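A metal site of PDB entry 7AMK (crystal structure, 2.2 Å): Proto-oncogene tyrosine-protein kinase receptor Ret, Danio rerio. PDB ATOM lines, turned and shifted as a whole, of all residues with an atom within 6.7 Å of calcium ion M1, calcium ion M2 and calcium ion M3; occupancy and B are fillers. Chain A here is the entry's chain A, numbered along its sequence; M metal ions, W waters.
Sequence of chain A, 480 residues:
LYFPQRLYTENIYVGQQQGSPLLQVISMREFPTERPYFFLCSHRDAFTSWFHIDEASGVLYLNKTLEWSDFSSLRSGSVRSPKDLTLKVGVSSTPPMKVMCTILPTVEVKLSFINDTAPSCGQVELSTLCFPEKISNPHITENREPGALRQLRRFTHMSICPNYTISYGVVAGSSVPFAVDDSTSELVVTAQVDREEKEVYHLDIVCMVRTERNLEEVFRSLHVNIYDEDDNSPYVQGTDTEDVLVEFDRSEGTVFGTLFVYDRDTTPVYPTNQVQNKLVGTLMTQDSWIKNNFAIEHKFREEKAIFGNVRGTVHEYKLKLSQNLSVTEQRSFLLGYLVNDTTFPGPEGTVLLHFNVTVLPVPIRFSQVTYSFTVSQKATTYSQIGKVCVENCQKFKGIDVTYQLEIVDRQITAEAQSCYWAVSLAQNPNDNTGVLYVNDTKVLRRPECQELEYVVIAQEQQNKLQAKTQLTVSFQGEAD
Seven residues have an atom within 4 Å of calcium ion M1: Glu 142, Glu 196, Asp 228, Glu 229, Asp 231, Asn 232 and Asp 265.
The nearest printed residue that does not touch calcium ion M1 is Arg 195 (4.6 Å).
The backbone NH (N) of Arg 195 lies close to the side-chain carboxylate (OE1) of Glu 142 (3.0 Å).
The side-chain carboxylate (OD1) of Asp 231 lies close to the side-chain amide nitrogen (ND2) of Asn 232, at 2.5 Å.
ND2 of Asn 277 sits at hydrogen-bond distance from O of Thr 266 (3.3 Å).
ND2 of Asn 232 lies close to OE1 of Glu 196 (3.3 Å).
The side-chain carboxylate (OD2) of Asp 230 is in hydrogen-bond range of the backbone NH (N) of Phe 344.
The backbone NH (N) of Thr 266 is in hydrogen-bond range of the side-chain carboxylate (OD2) of Asp 228, at 3.2 Å.
The backbone carbonyl oxygen of Asp 228 lies within hydrogen-bond range of the side-chain amide nitrogen of Gln 276, 3.1 Å away.
The side-chain carboxylate (OD1) of Asp 228 sits close to the guanidinium group (NE) of Arg 195, at 2.9 Å.
OE2 of Glu 142 is bound to calcium ion M1 (2.4 Å).
OD1 of Asp 265 binds calcium ion M1 (2.4 Å).
O of Glu 229 is bound to calcium ion M1.
Calcium ion M1 is bound by the side-chain carboxylate (OD1) of Asp 228.
OD1 of Asp 231 is bound to calcium ion M1 (2.5 Å).
Calcium ion M1 is bound by OE2 of Glu 196.
Calcium ion M1 is bound by the side-chain carboxylate (OE1) of Glu 196 (2.9 Å).
Within 4 Å of calcium ion M3: Asp 230, Asn 232, Asp 263, Asp 265, Asn 277 and Asp 341.
The backbone carbonyl oxygen (O) of Asn 232 is bound to calcium ion M3 (2.3 Å).
Calcium ion M3 is bound by OD1 of Asn 277 (2.3 Å).
The side-chain carboxylate (OD1) of Asp 230 is bound to calcium ion M3 (2.3 Å).
OD2 of Asp 265 binds calcium ion M3.
Calcium ion M3 is bound by OD2 of Asp 263.
The side-chain carboxylate (OD2) of Asp 341 binds calcium ion M3, at 2.5 Å.
Calcium ion M3 is bound by the side-chain carboxylate (OD1) of Asp 263 (2.6 Å).
Calcium ion M3 has seven donor atoms within binding distance.
Four residues have an atom within 4 Å of calcium ion M2: Glu 142, Asp 194, Glu 196 and Asp 231.
Calcium ion M2 is bound by the side-chain carboxylate of Asp 231 (2.3 Å), the side-chain carboxylate of Glu 142 (2.3 Å), the side-chain carboxylate of Asp 194 (2.3 Å), the side-chain carboxylate of Glu 196 (2.3 Å), water W1 (2.3 Å) and water W2 (2.3 Å).
Calcium ion M2 has six donor atoms within binding distance.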
ATOM      1  N   GLU A 142       9.430  21.861  21.310  1.00  0.00           N
ATOM      2  CA  GLU A 142       8.042  22.321  21.335  1.00  0.00           C
ATOM      3  C   GLU A 142       7.917  23.666  20.600  1.00  0.00           C
ATOM      4  O   GLU A 142       8.907  24.354  20.329  1.00  0.00           O
ATOM      5  CB  GLU A 142       7.580  22.426  22.804  1.00  0.00           C
ATOM      6  CG  GLU A 142       8.340  23.451  23.608  1.00  0.00           C
ATOM      7  CD  GLU A 142       7.682  23.819  24.927  1.00  0.00           C
ATOM      8  OE1 GLU A 142       6.485  23.536  25.130  1.00  0.00           O
ATOM      9  OE2 GLU A 142       8.401  24.385  25.764  1.00  0.00           O
ATOM     10  N   ASN A 143       6.674  24.006  20.231  1.00  0.00           N
ATOM     11  CA  ASN A 143       6.348  25.329  19.657  1.00  0.00           C
ATOM     12  C   ASN A 143       7.118  25.630  18.359  1.00  0.00           C
ATOM     13  O   ASN A 143       7.564  26.751  18.139  1.00  0.00           O
ATOM     14  CB  ASN A 143       6.592  26.470  20.646  1.00  0.00           C
ATOM     15  CG  ASN A 143       5.882  26.269  21.962  1.00  0.00           C
ATOM     16  OD1 ASN A 143       4.806  25.682  22.017  1.00  0.00           O
ATOM     17  ND2 ASN A 143       6.482  26.754  23.034  1.00  0.00           N
ATOM     18  N   VAL A 193       3.879  21.129  18.931  1.00  0.00           N
ATOM     19  CA  VAL A 193       3.569  20.333  20.111  1.00  0.00           C
ATOM     20  C   VAL A 193       3.928  21.147  21.367  1.00  0.00           C
ATOM     21  O   VAL A 193       4.513  22.225  21.289  1.00  0.00           O
ATOM     22  CB  VAL A 193       4.294  18.973  20.072  1.00  0.00           C
ATOM     23  CG1 VAL A 193       3.895  18.275  18.790  1.00  0.00           C
ATOM     24  CG2 VAL A 193       5.839  19.151  20.115  1.00  0.00           C
ATOM     25  N   ASP A 194       3.524  20.616  22.519  1.00  0.00           N
ATOM     26  CA  ASP A 194       3.647  21.312  23.805  1.00  0.00           C
ATOM     27  C   ASP A 194       4.349  20.366  24.760  1.00  0.00           C
ATOM     28  O   ASP A 194       3.791  19.342  25.174  1.00  0.00           O
ATOM     29  CB  ASP A 194       2.263  21.745  24.319  1.00  0.00           C
ATOM     30  CG  ASP A 194       2.308  22.479  25.690  1.00  0.00           C
ATOM     31  OD1 ASP A 194       3.403  22.826  26.171  1.00  0.00           O
ATOM     32  OD2 ASP A 194       1.238  22.678  26.304  1.00  0.00           O
ATOM     33  N   ARG A 195       5.605  20.692  25.090  1.00  0.00           N
ATOM     34  CA  ARG A 195       6.367  19.845  25.991  1.00  0.00           C
ATOM     35  C   ARG A 195       5.593  19.663  27.304  1.00  0.00           C
ATOM     36  O   ARG A 195       5.621  18.573  27.900  1.00  0.00           O
ATOM     37  CB  ARG A 195       7.752  20.448  26.237  1.00  0.00           C
ATOM     38  CG  ARG A 195       8.774  19.501  26.880  1.00  0.00           C
ATOM     39  CD  ARG A 195       8.497  19.179  28.352  1.00  0.00           C
ATOM     40  NE  ARG A 195       8.452  20.373  29.178  1.00  0.00           N
ATOM     41  CZ  ARG A 195       8.386  20.403  30.505  1.00  0.00           C
ATOM     42  NH1 ARG A 195       8.388  19.300  31.238  1.00  0.00           N
ATOM     43  NH2 ARG A 195       8.309  21.578  31.121  1.00  0.00           N
ATOM     44  N   GLU A 196       4.873  20.693  27.745  1.00  0.00           N
ATOM     45  CA  GLU A 196       4.130  20.623  29.001  1.00  0.00           C
ATOM     46  C   GLU A 196       2.928  19.702  28.919  1.00  0.00           C
ATOM     47  O   GLU A 196       2.405  19.271  29.956  1.00  0.00           O
ATOM     48  CB  GLU A 196       3.674  22.020  29.448  1.00  0.00           C
ATOM     49  CG  GLU A 196       4.738  22.821  30.237  1.00  0.00           C
ATOM     50  CD  GLU A 196       5.839  23.439  29.355  1.00  0.00           C
ATOM     51  OE1 GLU A 196       5.540  23.859  28.217  1.00  0.00           O
ATOM     52  OE2 GLU A 196       7.006  23.516  29.815  1.00  0.00           O
ATOM     53  N   GLU A 197       2.440  19.392  27.734  1.00  0.00           N
ATOM     54  CA  GLU A 197       1.390  18.393  27.636  1.00  0.00           C
ATOM     55  C   GLU A 197       1.973  17.000  27.535  1.00  0.00           C
ATOM     56  O   GLU A 197       1.487  16.080  28.201  1.00  0.00           O
ATOM     57  CB  GLU A 197       0.478  18.667  26.436  1.00  0.00           C
ATOM     58  N   TYR A 227      11.728  18.456  23.214  1.00  0.00           N
ATOM     59  CA  TYR A 227      12.569  19.378  23.968  1.00  0.00           C
ATOM     60  C   TYR A 227      11.799  20.618  24.383  1.00  0.00           C
ATOM     61  O   TYR A 227      10.885  21.075  23.706  1.00  0.00           O
ATOM     62  CB  TYR A 227      13.798  19.792  23.151  1.00  0.00           C
ATOM     63  CG  TYR A 227      14.823  18.698  23.017  1.00  0.00           C
ATOM     64  CD1 TYR A 227      14.636  17.443  23.592  1.00  0.00           C
ATOM     65  CD2 TYR A 227      15.997  18.927  22.324  1.00  0.00           C
ATOM     66  CE1 TYR A 227      15.602  16.437  23.470  1.00  0.00           C
ATOM     67  CE2 TYR A 227      16.961  17.949  22.196  1.00  0.00           C
ATOM     68  CZ  TYR A 227      16.760  16.704  22.759  1.00  0.00           C
ATOM     69  OH  TYR A 227      17.737  15.759  22.582  1.00  0.00           O
ATOM     70  N   ASP A 228      12.206  21.174  25.513  1.00  0.00           N
ATOM     71  CA  ASP A 228      11.505  22.244  26.191  1.00  0.00           C
ATOM     72  C   ASP A 228      12.073  23.575  25.758  1.00  0.00           C
ATOM     73  O   ASP A 228      13.266  23.716  25.475  1.00  0.00           O
ATOM     74  CB  ASP A 228      11.654  22.084  27.702  1.00  0.00           C
ATOM     75  CG  ASP A 228      10.810  23.034  28.481  1.00  0.00           C
ATOM     76  OD1 ASP A 228       9.585  22.962  28.339  1.00  0.00           O
ATOM     77  OD2 ASP A 228      11.357  23.833  29.257  1.00  0.00           O
ATOM     78  N   GLU A 229      11.218  24.579  25.725  1.00  0.00           N
ATOM     79  CA  GLU A 229      11.686  25.948  25.633  1.00  0.00           C
ATOM     80  C   GLU A 229      11.044  26.757  26.750  1.00  0.00           C
ATOM     81  O   GLU A 229      10.118  26.286  27.422  1.00  0.00           O
ATOM     82  CB  GLU A 229      11.397  26.554  24.258  1.00  0.00           C
ATOM     83  CG  GLU A 229       9.991  26.958  24.041  1.00  0.00           C
ATOM     84  CD  GLU A 229       9.819  27.689  22.718  1.00  0.00           C
ATOM     85  OE1 GLU A 229      10.806  27.756  21.951  1.00  0.00           O
ATOM     86  OE2 GLU A 229       8.706  28.202  22.420  1.00  0.00           O
ATOM     87  N   ASP A 230      11.560  27.959  26.972  1.00  0.00           N
ATOM     88  CA  ASP A 230      11.115  28.803  28.078  1.00  0.00           C
ATOM     89  C   ASP A 230       9.857  29.526  27.612  1.00  0.00           C
ATOM     90  O   ASP A 230       9.921  30.574  26.973  1.00  0.00           O
ATOM     91  CB  ASP A 230      12.238  29.755  28.504  1.00  0.00           C
ATOM     92  CG  ASP A 230      11.848  30.676  29.684  1.00  0.00           C
ATOM     93  OD1 ASP A 230      10.753  30.556  30.269  1.00  0.00           O
ATOM     94  OD2 ASP A 230      12.674  31.550  30.008  1.00  0.00           O
ATOM     95  N   ASP A 231       8.694  28.936  27.894  1.00  0.00           N
ATOM     96  CA  ASP A 231       7.433  29.508  27.431  1.00  0.00           C
ATOM     97  C   ASP A 231       6.427  29.604  28.571  1.00  0.00           C
ATOM     98  O   ASP A 231       5.217  29.673  28.314  1.00  0.00           O
ATOM     99  CB  ASP A 231       6.870  28.707  26.236  1.00  0.00           C
ATOM    100  CG  ASP A 231       6.453  27.262  26.621  1.00  0.00           C
ATOM    101  OD1 ASP A 231       6.654  26.827  27.774  1.00  0.00           O
ATOM    102  OD2 ASP A 231       5.907  26.562  25.741  1.00  0.00           O
ATOM    103  N   ASN A 232       6.891  29.600  29.817  1.00  0.00           N
ATOM    104  CA  ASN A 232       6.032  29.770  30.969  1.00  0.00           C
ATOM    105  C   ASN A 232       6.683  30.753  31.927  1.00  0.00           C
ATOM    106  O   ASN A 232       7.868  30.635  32.226  1.00  0.00           O
ATOM    107  CB  ASN A 232       5.773  28.433  31.676  1.00  0.00           C
ATOM    108  CG  ASN A 232       4.918  27.493  30.844  1.00  0.00           C
ATOM    109  OD1 ASN A 232       3.694  27.516  30.927  1.00  0.00           O
ATOM    110  ND2 ASN A 232       5.566  26.666  30.029  1.00  0.00           N
ATOM    111  N   SER A 233       5.901  31.749  32.387  1.00  0.00           N
ATOM    112  CA  SER A 233       6.468  32.692  33.314  1.00  0.00           C
ATOM    113  C   SER A 233       6.409  32.166  34.747  1.00  0.00           C
ATOM    114  O   SER A 233       5.538  31.367  35.083  1.00  0.00           O
ATOM    115  CB  SER A 233       5.736  34.020  33.247  1.00  0.00           C
ATOM    116  OG  SER A 233       4.351  33.818  33.392  1.00  0.00           O
ATOM    117  N   PRO A 234       7.345  32.609  35.578  1.00  0.00           N
ATOM    118  CA  PRO A 234       7.317  32.217  36.991  1.00  0.00           C
ATOM    119  C   PRO A 234       6.135  32.841  37.705  1.00  0.00           C
ATOM    120  O   PRO A 234       5.590  33.853  37.297  1.00  0.00           O
ATOM    121  CB  PRO A 234       8.646  32.758  37.518  1.00  0.00           C
ATOM    122  CG  PRO A 234       8.950  33.905  36.607  1.00  0.00           C
ATOM    123  CD  PRO A 234       8.499  33.452  35.259  1.00  0.00           C
ATOM    124  N   ASP A 263       7.911  27.503  38.178  1.00  0.00           N
ATOM    125  CA  ASP A 263       8.003  27.702  36.737  1.00  0.00           C
ATOM    126  C   ASP A 263       7.788  26.346  36.074  1.00  0.00           C
ATOM    127  O   ASP A 263       8.499  25.389  36.375  1.00  0.00           O
ATOM    128  CB  ASP A 263       9.369  28.300  36.358  1.00  0.00           C
ATOM    129  CG  ASP A 263       9.413  28.844  34.942  1.00  0.00           C
ATOM    130  OD1 ASP A 263       8.972  28.159  34.016  1.00  0.00           O
ATOM    131  OD2 ASP A 263       9.909  29.966  34.752  1.00  0.00           O
ATOM    132  N   ARG A 264       6.789  26.260  35.193  1.00  0.00           N
ATOM    133  CA  ARG A 264       6.466  24.975  34.577  1.00  0.00           C
ATOM    134  C   ARG A 264       7.546  24.487  33.618  1.00  0.00           C
ATOM    135  O   ARG A 264       7.580  23.286  33.306  1.00  0.00           O
ATOM    136  CB  ARG A 264       5.126  25.060  33.867  1.00  0.00           C
ATOM    137  CG  ARG A 264       3.997  25.333  34.845  1.00  0.00           C
ATOM    138  CD  ARG A 264       2.615  25.220  34.201  1.00  0.00           C
ATOM    139  NE  ARG A 264       1.579  25.466  35.204  1.00  0.00           N
ATOM    140  CZ  ARG A 264       1.082  24.554  36.033  1.00  0.00           C
ATOM    141  NH1 ARG A 264       1.478  23.296  35.986  1.00  0.00           N
ATOM    142  NH2 ARG A 264       0.168  24.924  36.924  1.00  0.00           N
ATOM    143  N   ASP A 265       8.412  25.372  33.149  1.00  0.00           N
ATOM    144  CA  ASP A 265       9.519  24.981  32.291  1.00  0.00           C
ATOM    145  C   ASP A 265      10.608  24.246  33.090  1.00  0.00           C
ATOM    146  O   ASP A 265      10.781  24.453  34.292  1.00  0.00           O
ATOM    147  CB  ASP A 265      10.122  26.205  31.605  1.00  0.00           C
ATOM    148  CG  ASP A 265       9.117  26.945  30.752  1.00  0.00           C
ATOM    149  OD1 ASP A 265       8.332  26.277  30.052  1.00  0.00           O
ATOM    150  OD2 ASP A 265       9.096  28.193  30.786  1.00  0.00           O
ATOM    151  N   THR A 266      11.344  23.391  32.393  1.00  0.00           N
ATOM    152  CA  THR A 266      12.477  22.672  32.963  1.00  0.00           C
ATOM    153  C   THR A 266      13.735  23.525  32.928  1.00  0.00           C
ATOM    154  O   THR A 266      13.850  24.499  32.182  1.00  0.00           O
ATOM    155  CB  THR A 266      12.747  21.360  32.191  1.00  0.00           C
ATOM    156  OG1 THR A 266      13.326  21.668  30.924  1.00  0.00           O
ATOM    157  CG2 THR A 266      11.452  20.595  31.982  1.00  0.00           C
ATOM    158  N   GLN A 276      18.867  29.449  29.321  1.00  0.00           N
ATOM    159  CA  GLN A 276      17.459  29.121  29.136  1.00  0.00           C
ATOM    160  C   GLN A 276      16.748  28.982  30.469  1.00  0.00           C
ATOM    161  O   GLN A 276      17.119  28.157  31.308  1.00  0.00           O
ATOM    162  CB  GLN A 276      17.310  27.823  28.336  1.00  0.00           C
ATOM    163  CG  GLN A 276      15.958  27.128  28.542  1.00  0.00           C
ATOM    164  CD  GLN A 276      15.648  26.041  27.511  1.00  0.00           C
ATOM    165  OE1 GLN A 276      16.370  25.858  26.518  1.00  0.00           O
ATOM    166  NE2 GLN A 276      14.552  25.316  27.731  1.00  0.00           N
ATOM    167  N   ASN A 277      15.706  29.783  30.659  1.00  0.00           N
ATOM    168  CA  ASN A 277      14.842  29.652  31.828  1.00  0.00           C
ATOM    169  C   ASN A 277      15.534  30.058  33.111  1.00  0.00           C
ATOM    170  O   ASN A 277      15.042  29.761  34.190  1.00  0.00           O
ATOM    171  CB  ASN A 277      14.299  28.232  31.993  1.00  0.00           C
ATOM    172  CG  ASN A 277      12.947  28.227  32.617  1.00  0.00           C
ATOM    173  OD1 ASN A 277      12.119  29.063  32.283  1.00  0.00           O
ATOM    174  ND2 ASN A 277      12.713  27.330  33.562  1.00  0.00           N
ATOM    175  N   LEU A 279      16.280  32.365  36.054  1.00  0.00           N
ATOM    176  CA  LEU A 279      15.724  33.511  36.754  1.00  0.00           C
ATOM    177  C   LEU A 279      16.852  34.273  37.459  1.00  0.00           C
ATOM    178  O   LEU A 279      17.582  33.699  38.257  1.00  0.00           O
ATOM    179  CB  LEU A 279      14.677  33.090  37.796  1.00  0.00           C
ATOM    180  CG  LEU A 279      13.509  32.203  37.346  1.00  0.00           C
ATOM    181  CD1 LEU A 279      12.559  31.936  38.537  1.00  0.00           C
ATOM    182  CD2 LEU A 279      12.812  32.889  36.204  1.00  0.00           C
ATOM    183  N   ASP A 341      12.488  36.148  34.760  1.00  0.00           N
ATOM    184  CA  ASP A 341      12.718  35.055  33.805  1.00  0.00           C
ATOM    185  C   ASP A 341      13.258  35.660  32.512  1.00  0.00           C
ATOM    186  O   ASP A 341      12.489  36.137  31.675  1.00  0.00           O
ATOM    187  CB  ASP A 341      11.437  34.281  33.556  1.00  0.00           C
ATOM    188  CG  ASP A 341      11.651  33.045  32.645  1.00  0.00           C
ATOM    189  OD1 ASP A 341      12.725  32.901  31.987  1.00  0.00           O
ATOM    190  OD2 ASP A 341      10.717  32.206  32.622  1.00  0.00           O
ATOM    191  N   THR A 343      14.771  34.783  29.605  1.00  0.00           N
ATOM    192  CA  THR A 343      14.456  34.302  28.273  1.00  0.00           C
ATOM    193  C   THR A 343      12.966  34.083  28.044  1.00  0.00           C
ATOM    194  O   THR A 343      12.591  33.471  27.039  1.00  0.00           O
ATOM    195  CB  THR A 343      15.217  32.987  27.977  1.00  0.00           C
ATOM    196  OG1 THR A 343      14.972  32.054  29.024  1.00  0.00           O
ATOM    197  CG2 THR A 343      16.707  33.233  27.913  1.00  0.00           C
ATOM    198  N   PHE A 344      12.106  34.520  28.961  1.00  0.00           N
ATOM    199  CA  PHE A 344      10.674  34.432  28.691  1.00  0.00           C
ATOM    200  C   PHE A 344      10.256  35.578  27.769  1.00  0.00           C
ATOM    201  O   PHE A 344      10.457  36.746  28.116  1.00  0.00           O
ATOM    202  CB  PHE A 344       9.858  34.451  29.969  1.00  0.00           C
ATOM    203  CG  PHE A 344       8.376  34.389  29.725  1.00  0.00           C
ATOM    204  CD1 PHE A 344       7.746  33.186  29.452  1.00  0.00           C
ATOM    205  CD2 PHE A 344       7.615  35.553  29.736  1.00  0.00           C
ATOM    206  CE1 PHE A 344       6.377  33.128  29.206  1.00  0.00           C
ATOM    207  CE2 PHE A 344       6.246  35.499  29.509  1.00  0.00           C
ATOM    208  CZ  PHE A 344       5.630  34.296  29.237  1.00  0.00           C
HETATM  209 CA    CA M   1       8.217  24.959  28.066  1.00  0.00          CA
HETATM  210 CA    CA M   2       4.799  24.641  26.192  1.00  0.00          CA
HETATM  211 CA    CA M   3       9.972  29.805  32.337  1.00  0.00          CA
HETATM  212  O   HOH W   1       3.880  25.043  24.092  1.00  0.00           O
HETATM  213  O   HOH W   2       3.192  25.820  27.411  1.00  0.00           O
